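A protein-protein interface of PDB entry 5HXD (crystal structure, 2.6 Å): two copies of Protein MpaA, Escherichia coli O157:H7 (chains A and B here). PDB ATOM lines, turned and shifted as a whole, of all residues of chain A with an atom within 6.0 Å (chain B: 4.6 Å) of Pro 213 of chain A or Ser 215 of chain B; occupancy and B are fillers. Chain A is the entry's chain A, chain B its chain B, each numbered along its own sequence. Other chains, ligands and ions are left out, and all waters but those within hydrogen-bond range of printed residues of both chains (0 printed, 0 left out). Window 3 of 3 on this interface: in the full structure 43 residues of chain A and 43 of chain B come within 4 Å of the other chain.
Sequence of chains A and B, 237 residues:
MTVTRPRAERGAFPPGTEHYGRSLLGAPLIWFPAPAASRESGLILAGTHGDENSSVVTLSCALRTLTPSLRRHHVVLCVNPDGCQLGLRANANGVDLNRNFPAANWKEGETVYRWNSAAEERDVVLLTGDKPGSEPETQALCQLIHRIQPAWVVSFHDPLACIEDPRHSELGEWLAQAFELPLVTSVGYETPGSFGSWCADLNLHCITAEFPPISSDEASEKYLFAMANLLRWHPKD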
ATOM      1  N   SER A 117      14.217  23.436  -9.927  1.00  0.00           N
ATOM      2  CA  SER A 117      12.775  23.733  -9.904  1.00  0.00           C
ATOM      3  C   SER A 117      12.419  24.968  -9.071  1.00  0.00           C
ATOM      4  O   SER A 117      11.405  25.630  -9.318  1.00  0.00           O
ATOM      5  CB  SER A 117      11.992  22.538  -9.374  1.00  0.00           C
ATOM      6  OG  SER A 117      12.286  22.325  -8.009  1.00  0.00           O
ATOM      7  N   ASP A 158      14.923  14.475 -15.917  1.00  0.00           N
ATOM      8  CA  ASP A 158      14.470  15.165 -14.688  1.00  0.00           C
ATOM      9  C   ASP A 158      14.204  16.636 -14.959  1.00  0.00           C
ATOM     10  O   ASP A 158      14.867  17.226 -15.812  1.00  0.00           O
ATOM     11  CB  ASP A 158      15.529  15.127 -13.584  1.00  0.00           C
ATOM     12  CG  ASP A 158      15.408  13.945 -12.700  1.00  0.00           C
ATOM     13  OD1 ASP A 158      14.432  13.184 -12.861  1.00  0.00           O
ATOM     14  OD2 ASP A 158      16.307  13.776 -11.848  1.00  0.00           O
ATOM     15  N   PRO A 159      13.297  17.264 -14.188  1.00  0.00           N
ATOM     16  CA  PRO A 159      12.378  16.690 -13.208  1.00  0.00           C
ATOM     17  C   PRO A 159      10.950  17.149 -13.492  1.00  0.00           C
ATOM     18  O   PRO A 159      10.231  17.503 -12.558  1.00  0.00           O
ATOM     19  CB  PRO A 159      12.889  17.287 -11.901  1.00  0.00           C
ATOM     20  CG  PRO A 159      13.435  18.696 -12.345  1.00  0.00           C
ATOM     21  CD  PRO A 159      13.499  18.687 -13.882  1.00  0.00           C
ATOM     22  N   LEU A 160      10.558  17.145 -14.765  1.00  0.00           N
ATOM     23  CA  LEU A 160       9.344  17.827 -15.190  1.00  0.00           C
ATOM     24  C   LEU A 160       8.074  16.998 -15.038  1.00  0.00           C
ATOM     25  O   LEU A 160       6.991  17.462 -15.404  1.00  0.00           O
ATOM     26  CB  LEU A 160       9.494  18.283 -16.635  1.00  0.00           C
ATOM     27  CG  LEU A 160      10.688  19.222 -16.762  1.00  0.00           C
ATOM     28  CD1 LEU A 160      10.785  19.721 -18.174  1.00  0.00           C
ATOM     29  CD2 LEU A 160      10.589  20.387 -15.770  1.00  0.00           C
ATOM     30  N   ALA A 161       8.216  15.788 -14.497  1.00  0.00           N
ATOM     31  CA  ALA A 161       7.080  14.986 -14.034  1.00  0.00           C
ATOM     32  C   ALA A 161       5.982  14.767 -15.088  1.00  0.00           C
ATOM     33  O   ALA A 161       4.804  15.053 -14.840  1.00  0.00           O
ATOM     34  CB  ALA A 161       6.477  15.618 -12.777  1.00  0.00           C
ATOM     35  N   PHE A 211      10.814  12.127 -15.228  1.00  0.00           N
ATOM     36  CA  PHE A 211      10.551  11.813 -13.834  1.00  0.00           C
ATOM     37  C   PHE A 211      10.145  13.073 -13.088  1.00  0.00           C
ATOM     38  O   PHE A 211      10.393  14.184 -13.548  1.00  0.00           O
ATOM     39  CB  PHE A 211      11.785  11.219 -13.176  1.00  0.00           C
ATOM     40  CG  PHE A 211      11.788   9.733 -13.112  1.00  0.00           C
ATOM     41  CD1 PHE A 211      10.970   8.983 -13.934  1.00  0.00           C
ATOM     42  CD2 PHE A 211      12.621   9.076 -12.216  1.00  0.00           C
ATOM     43  CE1 PHE A 211      10.988   7.592 -13.874  1.00  0.00           C
ATOM     44  CE2 PHE A 211      12.641   7.691 -12.140  1.00  0.00           C
ATOM     45  CZ  PHE A 211      11.823   6.947 -12.973  1.00  0.00           C
ATOM     46  N   PRO A 212       9.514  12.913 -11.924  1.00  0.00           N
ATOM     47  CA  PRO A 212       9.336  14.093 -11.076  1.00  0.00           C
ATOM     48  C   PRO A 212      10.582  14.254 -10.226  1.00  0.00           C
ATOM     49  O   PRO A 212      11.478  13.409 -10.331  1.00  0.00           O
ATOM     50  CB  PRO A 212       8.120  13.730 -10.236  1.00  0.00           C
ATOM     51  CG  PRO A 212       8.255  12.229 -10.063  1.00  0.00           C
ATOM     52  CD  PRO A 212       8.883  11.710 -11.348  1.00  0.00           C
ATOM     53  N   PRO A 213      10.664  15.323  -9.418  1.00  0.00           N
ATOM     54  CA  PRO A 213      11.748  15.319  -8.430  1.00  0.00           C
ATOM     55  C   PRO A 213      11.543  14.148  -7.486  1.00  0.00           C
ATOM     56  O   PRO A 213      10.467  14.006  -6.911  1.00  0.00           O
ATOM     57  CB  PRO A 213      11.586  16.653  -7.716  1.00  0.00           C
ATOM     58  CG  PRO A 213      10.868  17.521  -8.709  1.00  0.00           C
ATOM     59  CD  PRO A 213       9.925  16.597  -9.424  1.00  0.00           C
ATOM     60  N   ILE A 214      12.544  13.289  -7.375  1.00  0.00           N
ATOM     61  CA  ILE A 214      12.419  12.075  -6.588  1.00  0.00           C
ATOM     62  C   ILE A 214      13.795  11.438  -6.364  1.00  0.00           C
ATOM     63  O   ILE A 214      14.637  11.414  -7.261  1.00  0.00           O
ATOM     64  CB  ILE A 214      11.480  11.064  -7.271  1.00  0.00           C
ATOM     65  CG1 ILE A 214      11.232   9.867  -6.340  1.00  0.00           C
ATOM     66  CG2 ILE A 214      12.037  10.649  -8.651  1.00  0.00           C
ATOM     67  CD1 ILE A 214      10.364   8.769  -6.923  1.00  0.00           C
ATOM     68  N   SER A 215      14.023  10.932  -5.159  1.00  0.00           N
ATOM     69  CA  SER A 215      15.302  10.332  -4.821  1.00  0.00           C
ATOM     70  C   SER A 215      15.487   8.984  -5.507  1.00  0.00           C
ATOM     71  O   SER A 215      14.512   8.322  -5.800  1.00  0.00           O
ATOM     72  CB  SER A 215      15.409  10.167  -3.309  1.00  0.00           C
ATOM     73  OG  SER A 215      14.424   9.276  -2.834  1.00  0.00           O
ATOM     74  N   SER A 216      16.736   8.580  -5.742  1.00  0.00           N
ATOM     75  CA  SER A 216      17.053   7.244  -6.254  1.00  0.00           C
ATOM     76  C   SER A 216      16.602   6.122  -5.305  1.00  0.00           C
ATOM     77  O   SER A 216      16.561   4.952  -5.690  1.00  0.00           O
ATOM     78  CB  SER A 216      18.558   7.098  -6.511  1.00  0.00           C
ATOM     79  OG  SER A 216      19.120   8.294  -7.023  1.00  0.00           O
ATOM     80  N   SER B  54      22.689  12.259  -4.778  1.00  0.00           N
ATOM     81  CA  SER B  54      22.149  13.502  -4.279  1.00  0.00           C
ATOM     82  C   SER B  54      23.314  14.288  -3.697  1.00  0.00           C
ATOM     83  O   SER B  54      23.384  15.511  -3.811  1.00  0.00           O
ATOM     84  CB  SER B  54      21.055  13.247  -3.233  1.00  0.00           C
ATOM     85  OG  SER B  54      21.429  12.212  -2.329  1.00  0.00           O
ATOM     86  N   ILE B 214      16.643  11.952  -0.890  1.00  0.00           N
ATOM     87  CA  ILE B 214      16.273  13.253  -1.450  1.00  0.00           C
ATOM     88  C   ILE B 214      16.660  13.366  -2.930  1.00  0.00           C
ATOM     89  O   ILE B 214      17.677  12.833  -3.384  1.00  0.00           O
ATOM     90  CB  ILE B 214      16.916  14.426  -0.645  1.00  0.00           C
ATOM     91  CG1 ILE B 214      16.277  15.771  -1.010  1.00  0.00           C
ATOM     92  CG2 ILE B 214      18.429  14.479  -0.841  1.00  0.00           C
ATOM     93  CD1 ILE B 214      16.849  16.935  -0.241  1.00  0.00           C
ATOM     94  N   SER B 215      15.810  14.040  -3.690  1.00  0.00           N
ATOM     95  CA  SER B 215      16.062  14.234  -5.097  1.00  0.00           C
ATOM     96  C   SER B 215      17.282  15.134  -5.269  1.00  0.00           C
ATOM     97  O   SER B 215      17.611  15.917  -4.377  1.00  0.00           O
ATOM     98  CB  SER B 215      14.837  14.840  -5.779  1.00  0.00           C
ATOM     99  OG  SER B 215      14.651  16.197  -5.423  1.00  0.00           O
ATOM    100  N   SER B 216      17.960  15.012  -6.403  1.00  0.00           N
ATOM    101  CA  SER B 216      19.008  15.957  -6.746  1.00  0.00           C
ATOM    102  C   SER B 216      18.404  17.342  -6.874  1.00  0.00           C
ATOM    103  O   SER B 216      19.078  18.344  -6.599  1.00  0.00           O
ATOM    104  CB  SER B 216      19.714  15.570  -8.048  1.00  0.00           C
ATOM    105  OG  SER B 216      20.586  14.476  -7.835  1.00  0.00           O
ATOM    106  N   ASP B 217      17.136  17.399  -7.280  1.00  0.00           N
ATOM    107  CA  ASP B 217      16.463  18.676  -7.487  1.00  0.00           C
ATOM    108  C   ASP B 217      16.168  19.414  -6.177  1.00  0.00           C
ATOM    109  O   ASP B 217      16.159  20.649  -6.140  1.00  0.00           O
ATOM    110  CB  ASP B 217      15.153  18.485  -8.253  1.00  0.00           C
ATOM    111  CG  ASP B 217      14.366  19.784  -8.382  1.00  0.00           C
ATOM    112  OD1 ASP B 217      14.815  20.679  -9.136  1.00  0.00           O
ATOM    113  OD2 ASP B 217      13.321  19.921  -7.699  1.00  0.00           O
ATOM    114  N   GLU B 218      15.908  18.677  -5.104  1.00  0.00           N
ATOM    115  CA  GLU B 218      15.577  19.334  -3.857  1.00  0.00           C
ATOM    116  C   GLU B 218      16.858  19.702  -3.108  1.00  0.00           C
ATOM    117  O   GLU B 218      16.980  20.818  -2.587  1.00  0.00           O
ATOM    118  CB  GLU B 218      14.678  18.452  -2.992  1.00  0.00           C
ATOM    119  CG  GLU B 218      14.048  19.215  -1.836  1.00  0.00           C
ATOM    120  CD  GLU B 218      13.271  18.332  -0.890  1.00  0.00           C
ATOM    121  OE1 GLU B 218      13.199  17.106  -1.130  1.00  0.00           O
ATOM    122  OE2 GLU B 218      12.740  18.875   0.099  1.00  0.00           O
ATOM    123  N   ALA B 219      17.802  18.759  -3.082  1.00  0.00           N
ATOM    124  CA  ALA B 219      19.079  18.895  -2.380  1.00  0.00           C
ATOM    125  C   ALA B 219      19.917  20.090  -2.873  1.00  0.00           C
ATOM    126  O   ALA B 219      20.484  20.845  -2.076  1.00  0.00           O
ATOM    127  CB  ALA B 219      19.869  17.592  -2.510  1.00  0.00           C
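Ser 215 of chain B touches just these residues of chain A: Pro 213 (3.8 Å), Ile 214 (3.2 Å) and Ser 215 (3.9 Å). Printed residues of chain A within 4 Å of Asp 217 of chain B: Ser 117 and Pro 213. Of the printed residues of chain A, Ile 214 of chain B touches Ser 215 (3.2 Å). Of the printed residues of chain B, Ile 214 of chain A touches Ser 215 (3.2 Å). Pro 159 of chain A touches none of the printed residues of chain B. The nearest printed residue of chain B that does not touch Pro 213 of chain A is Glu 218 of chain B (5.4 Å). The nearest residue of chain A that does not touch Ser 215 of chain B is Ser 216 of chain A (5.7 Å).
Ile 214 of chain A touches Ser 215 of chain B, and with the chains exchanged Ser 215 of chain A touches Ile 214 of chain B. Ser 215 of chain B touches its own counterpart, Ser 215 of chain A. Positions printed for both chains: 214, 215 and 216. Of the 6 pairs that touch across the chains among the printed residues, 3 have their exchanged pair printed and touching as well.
OG of Ser 117 of chain A is in hydrogen-bond range of OD2 of Asp 217 of chain B (2.6 Å).
The backbone NH of Asp 217 of chain B lies close to the side-chain hydroxyl of Ser 215 of chain B (3.3 Å). The backbone NH (N) of Glu 218 of chain B lies within hydrogen-bond range of the side-chain hydroxyl (OG) of Ser 215 of chain B (2.8 Å).
Of the 7 printed residues of chain B, 3 touch a printed residue of chain A. Of the 11 printed residues of chain A, 4 touch a printed residue of chain B. Among the printed residues, no Asp or Glu carboxylate lies within 4 Å of a Lys or Arg side-chain nitrogen of the other chain.
Ser 215 of chain B touches Pro 213 of chain A (CB to C, 3.8 Å). CG of Pro 213 of chain A touches OD2 of Asp 217 of chain B (3.6 Å). Ile 214 of chain A touches Ser 215 of chain B. N of Ile 214 of chain B touches CB of Ser 215 of chain A, 3.2 Å away. Ser 215 of chain B touches Ser 215 of chain A.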
